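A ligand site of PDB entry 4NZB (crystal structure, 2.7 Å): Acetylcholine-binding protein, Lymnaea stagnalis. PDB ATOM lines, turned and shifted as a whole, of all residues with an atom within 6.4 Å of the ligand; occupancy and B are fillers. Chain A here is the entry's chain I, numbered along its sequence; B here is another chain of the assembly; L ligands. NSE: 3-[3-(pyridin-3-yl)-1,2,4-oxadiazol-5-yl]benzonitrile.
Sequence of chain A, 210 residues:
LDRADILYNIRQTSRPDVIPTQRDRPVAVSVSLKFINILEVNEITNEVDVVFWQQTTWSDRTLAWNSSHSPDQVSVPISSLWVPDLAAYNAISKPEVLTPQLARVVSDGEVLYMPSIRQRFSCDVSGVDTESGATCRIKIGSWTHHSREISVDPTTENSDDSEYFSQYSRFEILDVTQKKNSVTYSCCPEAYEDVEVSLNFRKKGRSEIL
O of Trp 143 sits close to N2 of the ligand (3.5 Å). Residues that only touch the ligand: Leu 112 of chain B, Trp 53 of chain B, Arg 104 of chain B and Met 114 of chain B. Eight residues have an atom within 4 Å of the ligand: Tyr 89, Trp 143, Tyr 185, Tyr 192, Trp 53 of chain B, Arg 104 of chain B, Leu 112 of chain B and Met 114 of chain B. The nearest printed residue that does not touch the ligand is Thr 144 (4.04 Å).
O of Leu 112 of chain B is in hydrogen-bond range of N of Arg 104 of chain B (2.8 Å). NE of Arg 104 of chain B is in hydrogen-bond range of OE1 of Gln 73 of chain B (2.8 Å). The backbone NH of Tyr 192 sits at hydrogen-bond distance from the backbone carbonyl oxygen of Val 183, 2.7 Å away. O of Thr 144 sits at hydrogen-bond distance from NH1 of Arg 104 of chain B, at 3.2 Å. The indole nitrogen (NE1) of Trp 143 sits at hydrogen-bond distance from the backbone carbonyl oxygen (O) of Met 114 of chain B (3.1 Å).
OH of Tyr 89 lies within hydrogen-bond range of N4 of the ligand (3.3 Å). N4 of the ligand lies close to OH of Tyr 185 (3.4 Å). N1 of the ligand sits at hydrogen-bond distance from OH of Tyr 192.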
ATOM      1  N   TYR A  89      18.209 -15.183 -18.421  1.00  0.00           N
ATOM      2  CA  TYR A  89      19.160 -14.238 -17.847  1.00  0.00           C
ATOM      3  C   TYR A  89      19.981 -14.832 -16.692  1.00  0.00           C
ATOM      4  O   TYR A  89      21.147 -14.479 -16.522  1.00  0.00           O
ATOM      5  CB  TYR A  89      18.430 -12.969 -17.365  1.00  0.00           C
ATOM      6  CG  TYR A  89      17.737 -12.211 -18.456  1.00  0.00           C
ATOM      7  CD1 TYR A  89      18.070 -12.407 -19.778  1.00  0.00           C
ATOM      8  CD2 TYR A  89      16.736 -11.307 -18.181  1.00  0.00           C
ATOM      9  CE1 TYR A  89      17.442 -11.733 -20.792  1.00  0.00           C
ATOM     10  CE2 TYR A  89      16.087 -10.626 -19.183  1.00  0.00           C
ATOM     11  CZ  TYR A  89      16.448 -10.833 -20.486  1.00  0.00           C
ATOM     12  OH  TYR A  89      15.805 -10.153 -21.510  1.00  0.00           O
ATOM     13  N   SER A 142      14.367 -11.756 -25.034  1.00  0.00           N
ATOM     14  CA  SER A 142      15.217 -11.659 -26.205  1.00  0.00           C
ATOM     15  C   SER A 142      16.573 -11.163 -25.775  1.00  0.00           C
ATOM     16  O   SER A 142      16.661 -10.299 -24.911  1.00  0.00           O
ATOM     17  CB  SER A 142      14.632 -10.730 -27.262  1.00  0.00           C
ATOM     18  OG  SER A 142      15.627 -10.323 -28.175  1.00  0.00           O
ATOM     19  N   TRP A 143      17.629 -11.701 -26.371  1.00  0.00           N
ATOM     20  CA  TRP A 143      18.979 -11.308 -25.969  1.00  0.00           C
ATOM     21  C   TRP A 143      19.420 -10.003 -26.645  1.00  0.00           C
ATOM     22  O   TRP A 143      20.192  -9.245 -26.080  1.00  0.00           O
ATOM     23  CB  TRP A 143      19.976 -12.426 -26.261  1.00  0.00           C
ATOM     24  CG  TRP A 143      21.338 -12.148 -25.700  1.00  0.00           C
ATOM     25  CD1 TRP A 143      22.468 -11.870 -26.403  1.00  0.00           C
ATOM     26  CD2 TRP A 143      21.688 -12.096 -24.317  1.00  0.00           C
ATOM     27  NE1 TRP A 143      23.519 -11.652 -25.536  1.00  0.00           N
ATOM     28  CE2 TRP A 143      23.053 -11.785 -24.245  1.00  0.00           C
ATOM     29  CE3 TRP A 143      20.971 -12.276 -23.133  1.00  0.00           C
ATOM     30  CZ2 TRP A 143      23.727 -11.653 -23.042  1.00  0.00           C
ATOM     31  CZ3 TRP A 143      21.643 -12.157 -21.935  1.00  0.00           C
ATOM     32  CH2 TRP A 143      23.001 -11.842 -21.894  1.00  0.00           C
ATOM     33  N   THR A 144      18.928  -9.737 -27.855  1.00  0.00           N
ATOM     34  CA  THR A 144      19.386  -8.568 -28.604  1.00  0.00           C
ATOM     35  C   THR A 144      18.270  -7.686 -29.151  1.00  0.00           C
ATOM     36  O   THR A 144      18.522  -6.581 -29.639  1.00  0.00           O
ATOM     37  CB  THR A 144      20.290  -8.977 -29.785  1.00  0.00           C
ATOM     38  OG1 THR A 144      19.517  -9.618 -30.818  1.00  0.00           O
ATOM     39  CG2 THR A 144      21.404  -9.914 -29.312  1.00  0.00           C
ATOM     40  N   HIS A 145      17.025  -8.162 -29.091  1.00  0.00           N
ATOM     41  CA  HIS A 145      15.912  -7.379 -29.622  1.00  0.00           C
ATOM     42  C   HIS A 145      15.140  -6.684 -28.514  1.00  0.00           C
ATOM     43  O   HIS A 145      14.881  -7.280 -27.481  1.00  0.00           O
ATOM     44  CB  HIS A 145      14.975  -8.262 -30.440  1.00  0.00           C
ATOM     45  CG  HIS A 145      15.595  -8.822 -31.670  1.00  0.00           C
ATOM     46  ND1 HIS A 145      15.737  -8.095 -32.847  1.00  0.00           N
ATOM     47  CD2 HIS A 145      16.117 -10.044 -31.944  1.00  0.00           C
ATOM     48  CE1 HIS A 145      16.288  -8.841 -33.764  1.00  0.00           C
ATOM     49  NE2 HIS A 145      16.539 -10.037 -33.251  1.00  0.00           N
ATOM     50  N   HIS A 146      14.763  -5.429 -28.739  1.00  0.00           N
ATOM     51  CA  HIS A 146      13.957  -4.687 -27.763  1.00  0.00           C
ATOM     52  C   HIS A 146      12.450  -4.829 -28.029  1.00  0.00           C
ATOM     53  O   HIS A 146      12.024  -5.449 -28.996  1.00  0.00           O
ATOM     54  CB  HIS A 146      14.383  -3.214 -27.755  1.00  0.00           C
ATOM     55  CG  HIS A 146      14.327  -2.555 -29.089  1.00  0.00           C
ATOM     56  ND1 HIS A 146      13.141  -2.287 -29.741  1.00  0.00           N
ATOM     57  CD2 HIS A 146      15.310  -2.102 -29.899  1.00  0.00           C
ATOM     58  CE1 HIS A 146      13.394  -1.705 -30.897  1.00  0.00           C
ATOM     59  NE2 HIS A 146      14.703  -1.572 -31.021  1.00  0.00           N
ATOM     60  N   VAL A 183      11.604  -3.602 -19.020  1.00  0.00           N
ATOM     61  CA  VAL A 183      12.668  -2.864 -18.363  1.00  0.00           C
ATOM     62  C   VAL A 183      13.357  -1.856 -19.288  1.00  0.00           C
ATOM     63  O   VAL A 183      13.757  -2.210 -20.400  1.00  0.00           O
ATOM     64  CB  VAL A 183      13.734  -3.811 -17.788  1.00  0.00           C
ATOM     65  CG1 VAL A 183      14.626  -3.016 -16.940  1.00  0.00           C
ATOM     66  CG2 VAL A 183      13.115  -4.872 -16.925  1.00  0.00           C
ATOM     67  N   TYR A 185      16.550   0.774 -19.554  1.00  0.00           N
ATOM     68  CA  TYR A 185      17.783   1.128 -18.869  1.00  0.00           C
ATOM     69  C   TYR A 185      18.240   2.530 -19.187  1.00  0.00           C
ATOM     70  O   TYR A 185      17.575   3.247 -19.919  1.00  0.00           O
ATOM     71  CB  TYR A 185      18.963   0.158 -19.114  1.00  0.00           C
ATOM     72  CG  TYR A 185      18.681  -1.331 -19.008  1.00  0.00           C
ATOM     73  CD1 TYR A 185      17.363  -1.844 -18.866  1.00  0.00           C
ATOM     74  CD2 TYR A 185      19.770  -2.198 -18.669  1.00  0.00           C
ATOM     75  CE1 TYR A 185      17.143  -3.131 -18.694  1.00  0.00           C
ATOM     76  CE2 TYR A 185      19.556  -3.525 -18.415  1.00  0.00           C
ATOM     77  CZ  TYR A 185      18.202  -4.003 -18.411  1.00  0.00           C
ATOM     78  OH  TYR A 185      17.849  -5.342 -18.174  1.00  0.00           O
ATOM     79  N   TYR A 192      13.173  -3.476 -22.759  1.00  0.00           N
ATOM     80  CA  TYR A 192      13.446  -4.888 -22.969  1.00  0.00           C
ATOM     81  C   TYR A 192      12.525  -5.733 -22.093  1.00  0.00           C
ATOM     82  O   TYR A 192      12.547  -5.637 -20.869  1.00  0.00           O
ATOM     83  CB  TYR A 192      14.919  -5.216 -22.678  1.00  0.00           C
ATOM     84  CG  TYR A 192      15.857  -4.563 -23.659  1.00  0.00           C
ATOM     85  CD1 TYR A 192      16.242  -3.233 -23.503  1.00  0.00           C
ATOM     86  CD2 TYR A 192      16.337  -5.256 -24.770  1.00  0.00           C
ATOM     87  CE1 TYR A 192      17.085  -2.620 -24.404  1.00  0.00           C
ATOM     88  CE2 TYR A 192      17.179  -4.639 -25.681  1.00  0.00           C
ATOM     89  CZ  TYR A 192      17.550  -3.321 -25.487  1.00  0.00           C
ATOM     90  OH  TYR A 192      18.386  -2.705 -26.376  1.00  0.00           O
ATOM     91  N   GLU A 193      11.703  -6.530 -22.737  1.00  0.00           N
ATOM     92  CA  GLU A 193      10.731  -7.342 -22.031  1.00  0.00           C
ATOM     93  C   GLU A 193      11.301  -8.691 -21.668  1.00  0.00           C
ATOM     94  O   GLU A 193      12.194  -9.201 -22.341  1.00  0.00           O
ATOM     95  CB  GLU A 193       9.477  -7.528 -22.888  1.00  0.00           C
ATOM     96  CG  GLU A 193       8.909  -6.240 -23.413  1.00  0.00           C
ATOM     97  CD  GLU A 193       7.613  -6.447 -24.161  1.00  0.00           C
ATOM     98  OE1 GLU A 193       7.231  -7.626 -24.356  1.00  0.00           O
ATOM     99  OE2 GLU A 193       6.971  -5.458 -24.554  1.00  0.00           O
ATOM    100  N   ASP A 194      10.783  -9.262 -20.586  1.00  0.00           N
ATOM    101  CA  ASP A 194      11.107 -10.635 -20.236  1.00  0.00           C
ATOM    102  C   ASP A 194       9.890 -11.268 -19.614  1.00  0.00           C
ATOM    103  O   ASP A 194       8.961 -10.566 -19.212  1.00  0.00           O
ATOM    104  CB  ASP A 194      12.313 -10.700 -19.282  1.00  0.00           C
ATOM    105  CG  ASP A 194      12.035 -10.051 -17.927  1.00  0.00           C
ATOM    106  OD1 ASP A 194      11.346 -10.674 -17.092  1.00  0.00           O
ATOM    107  OD2 ASP A 194      12.541  -8.918 -17.695  1.00  0.00           O
ATOM    108  N   TRP B  53      29.283 -11.212 -18.556  1.00  0.00           N
ATOM    109  CA  TRP B  53      28.897 -10.691 -19.851  1.00  0.00           C
ATOM    110  C   TRP B  53      30.057  -9.895 -20.422  1.00  0.00           C
ATOM    111  O   TRP B  53      30.455  -8.864 -19.865  1.00  0.00           O
ATOM    112  CB  TRP B  53      27.635  -9.833 -19.745  1.00  0.00           C
ATOM    113  CG  TRP B  53      26.436 -10.586 -19.234  1.00  0.00           C
ATOM    114  CD1 TRP B  53      26.329 -11.936 -19.073  1.00  0.00           C
ATOM    115  CD2 TRP B  53      25.190 -10.031 -18.816  1.00  0.00           C
ATOM    116  NE1 TRP B  53      25.094 -12.268 -18.573  1.00  0.00           N
ATOM    117  CE2 TRP B  53      24.369 -11.106 -18.410  1.00  0.00           C
ATOM    118  CE3 TRP B  53      24.685  -8.736 -18.738  1.00  0.00           C
ATOM    119  CZ2 TRP B  53      23.074 -10.927 -17.932  1.00  0.00           C
ATOM    120  CZ3 TRP B  53      23.390  -8.550 -18.278  1.00  0.00           C
ATOM    121  CH2 TRP B  53      22.603  -9.639 -17.867  1.00  0.00           C
ATOM    122  N   GLN B  73      19.241  -0.047 -36.523  1.00  0.00           N
ATOM    123  CA  GLN B  73      20.019  -1.179 -36.021  1.00  0.00           C
ATOM    124  C   GLN B  73      19.445  -2.525 -36.453  1.00  0.00           C
ATOM    125  O   GLN B  73      18.247  -2.647 -36.697  1.00  0.00           O
ATOM    126  CB  GLN B  73      20.077  -1.168 -34.487  1.00  0.00           C
ATOM    127  CG  GLN B  73      20.618   0.090 -33.854  1.00  0.00           C
ATOM    128  CD  GLN B  73      20.688  -0.028 -32.347  1.00  0.00           C
ATOM    129  OE1 GLN B  73      20.380  -1.088 -31.779  1.00  0.00           O
ATOM    130  NE2 GLN B  73      21.109   1.049 -31.677  1.00  0.00           N
ATOM    131  N   LEU B 102      24.632 -13.554 -31.482  1.00  0.00           N
ATOM    132  CA  LEU B 102      24.292 -12.414 -32.338  1.00  0.00           C
ATOM    133  C   LEU B 102      24.997 -11.169 -31.889  1.00  0.00           C
ATOM    134  O   LEU B 102      25.282 -11.013 -30.714  1.00  0.00           O
ATOM    135  CB  LEU B 102      22.784 -12.155 -32.335  1.00  0.00           C
ATOM    136  CG  LEU B 102      21.864 -13.316 -32.690  1.00  0.00           C
ATOM    137  CD1 LEU B 102      20.415 -12.910 -32.513  1.00  0.00           C
ATOM    138  CD2 LEU B 102      22.107 -13.762 -34.128  1.00  0.00           C
ATOM    139  N   ALA B 103      25.282 -10.270 -32.807  1.00  0.00           N
ATOM    140  CA  ALA B 103      25.820  -8.976 -32.427  1.00  0.00           C
ATOM    141  C   ALA B 103      24.821  -7.913 -32.872  1.00  0.00           C
ATOM    142  O   ALA B 103      23.996  -8.141 -33.750  1.00  0.00           O
ATOM    143  CB  ALA B 103      27.174  -8.740 -33.058  1.00  0.00           C
ATOM    144  N   ARG B 104      24.888  -6.745 -32.258  1.00  0.00           N
ATOM    145  CA  ARG B 104      23.996  -5.656 -32.606  1.00  0.00           C
ATOM    146  C   ARG B 104      24.758  -4.652 -33.467  1.00  0.00           C
ATOM    147  O   ARG B 104      25.788  -4.133 -33.064  1.00  0.00           O
ATOM    148  CB  ARG B 104      23.444  -5.012 -31.343  1.00  0.00           C
ATOM    149  CG  ARG B 104      22.312  -4.048 -31.559  1.00  0.00           C
ATOM    150  CD  ARG B 104      21.019  -4.770 -31.860  1.00  0.00           C
ATOM    151  NE  ARG B 104      19.941  -3.825 -32.126  1.00  0.00           N
ATOM    152  CZ  ARG B 104      18.706  -4.158 -32.504  1.00  0.00           C
ATOM    153  NH1 ARG B 104      18.384  -5.432 -32.670  1.00  0.00           N
ATOM    154  NH2 ARG B 104      17.801  -3.215 -32.705  1.00  0.00           N
ATOM    155  N   LEU B 112      28.110  -4.002 -31.369  1.00  0.00           N
ATOM    156  CA  LEU B 112      28.130  -4.440 -29.984  1.00  0.00           C
ATOM    157  C   LEU B 112      27.917  -5.948 -29.895  1.00  0.00           C
ATOM    158  O   LEU B 112      26.881  -6.452 -30.313  1.00  0.00           O
ATOM    159  CB  LEU B 112      27.059  -3.724 -29.171  1.00  0.00           C
ATOM    160  CG  LEU B 112      26.716  -4.340 -27.794  1.00  0.00           C
ATOM    161  CD1 LEU B 112      27.877  -4.198 -26.805  1.00  0.00           C
ATOM    162  CD2 LEU B 112      25.451  -3.760 -27.195  1.00  0.00           C
ATOM    163  N   TYR B 113      28.897  -6.655 -29.358  1.00  0.00           N
ATOM    164  CA  TYR B 113      28.774  -8.092 -29.145  1.00  0.00           C
ATOM    165  C   TYR B 113      28.956  -8.340 -27.654  1.00  0.00           C
ATOM    166  O   TYR B 113      30.002  -8.024 -27.103  1.00  0.00           O
ATOM    167  CB  TYR B 113      29.809  -8.870 -29.982  1.00  0.00           C
ATOM    168  CG  TYR B 113      29.838 -10.350 -29.750  1.00  0.00           C
ATOM    169  CD1 TYR B 113      28.665 -11.101 -29.773  1.00  0.00           C
ATOM    170  CD2 TYR B 113      31.040 -11.023 -29.540  1.00  0.00           C
ATOM    171  CE1 TYR B 113      28.691 -12.479 -29.567  1.00  0.00           C
ATOM    172  CE2 TYR B 113      31.073 -12.411 -29.328  1.00  0.00           C
ATOM    173  CZ  TYR B 113      29.890 -13.118 -29.344  1.00  0.00           C
ATOM    174  OH  TYR B 113      29.913 -14.472 -29.140  1.00  0.00           O
ATOM    175  N   MET B 114      27.936  -8.886 -27.008  1.00  0.00           N
ATOM    176  CA  MET B 114      27.954  -9.063 -25.567  1.00  0.00           C
ATOM    177  C   MET B 114      27.471 -10.457 -25.181  1.00  0.00           C
ATOM    178  O   MET B 114      26.367 -10.646 -24.701  1.00  0.00           O
ATOM    179  CB  MET B 114      27.108  -7.982 -24.869  1.00  0.00           C
ATOM    180  CG  MET B 114      27.065  -8.096 -23.330  1.00  0.00           C
ATOM    181  SD  MET B 114      26.698  -6.594 -22.403  1.00  0.00           S
ATOM    182  CE  MET B 114      25.935  -5.552 -23.654  1.00  0.00           C
ATOM    183  N   PRO B 115      28.337 -11.450 -25.375  1.00  0.00           N
ATOM    184  CA  PRO B 115      27.950 -12.812 -25.008  1.00  0.00           C
ATOM    185  C   PRO B 115      28.030 -13.024 -23.515  1.00  0.00           C
ATOM    186  O   PRO B 115      28.770 -12.325 -22.824  1.00  0.00           O
ATOM    187  CB  PRO B 115      28.978 -13.672 -25.748  1.00  0.00           C
ATOM    188  CG  PRO B 115      30.192 -12.792 -25.837  1.00  0.00           C
ATOM    189  CD  PRO B 115      29.676 -11.400 -26.012  1.00  0.00           C
ATOM    190  N   TYR B 164      24.899  -6.279 -12.148  1.00  0.00           N
ATOM    191  CA  TYR B 164      24.134  -7.401 -12.700  1.00  0.00           C
ATOM    192  C   TYR B 164      24.495  -8.692 -11.976  1.00  0.00           C
ATOM    193  O   TYR B 164      24.115  -9.779 -12.414  1.00  0.00           O
ATOM    194  CB  TYR B 164      24.516  -7.456 -14.149  1.00  0.00           C
ATOM    195  CG  TYR B 164      23.992  -6.307 -15.004  1.00  0.00           C
ATOM    196  CD1 TYR B 164      22.699  -5.764 -14.923  1.00  0.00           C
ATOM    197  CD2 TYR B 164      24.963  -5.524 -15.636  1.00  0.00           C
ATOM    198  CE1 TYR B 164      22.372  -4.664 -15.676  1.00  0.00           C
ATOM    199  CE2 TYR B 164      24.654  -4.412 -16.310  1.00  0.00           C
ATOM    200  CZ  TYR B 164      23.361  -3.952 -16.367  1.00  0.00           C
ATOM    201  OH  TYR B 164      23.049  -2.791 -17.107  1.00  0.00           O
HETATM  202  C4  NSE L   1      21.574  -4.080 -27.593  1.00  0.00           C
HETATM  203  C14 NSE L   1      17.785  -7.802 -19.641  1.00  0.00           C
HETATM  204  C5  NSE L   1      21.852  -5.698 -25.763  1.00  0.00           C
HETATM  205  C6  NSE L   1      23.344  -7.621 -26.055  1.00  0.00           C
HETATM  206  C11 NSE L   1      21.093  -7.711 -22.151  1.00  0.00           C
HETATM  207  C7  NSE L   1      22.092  -7.283 -23.922  1.00  0.00           C
HETATM  208  C8  NSE L   1      22.455  -6.865 -25.267  1.00  0.00           C
HETATM  209  C9  NSE L   1      19.984  -7.758 -21.221  1.00  0.00           C
HETATM  210  C10 NSE L   1      18.720  -7.414 -21.706  1.00  0.00           C
HETATM  211  C12 NSE L   1      20.137  -8.151 -19.881  1.00  0.00           C
HETATM  212  C13 NSE L   1      19.014  -8.167 -19.068  1.00  0.00           C
HETATM  213  N1  NSE L   1      21.111  -3.118 -28.058  1.00  0.00           N
HETATM  214  N2  NSE L   1      20.920  -7.153 -23.396  1.00  0.00           N
HETATM  215  C3  NSE L   1      22.160  -5.277 -27.054  1.00  0.00           C
HETATM  216  N3  NSE L   1      22.315  -8.166 -21.901  1.00  0.00           N
HETATM  217  N4  NSE L   1      17.634  -7.418 -20.920  1.00  0.00           N
HETATM  218  O1  NSE L   1      22.993  -7.889 -23.102  1.00  0.00           O
HETATM  219  C2  NSE L   1      23.646  -7.190 -27.352  1.00  0.00           C
HETATM  220  C1  NSE L   1      23.049  -6.029 -27.851  1.00  0.00           C
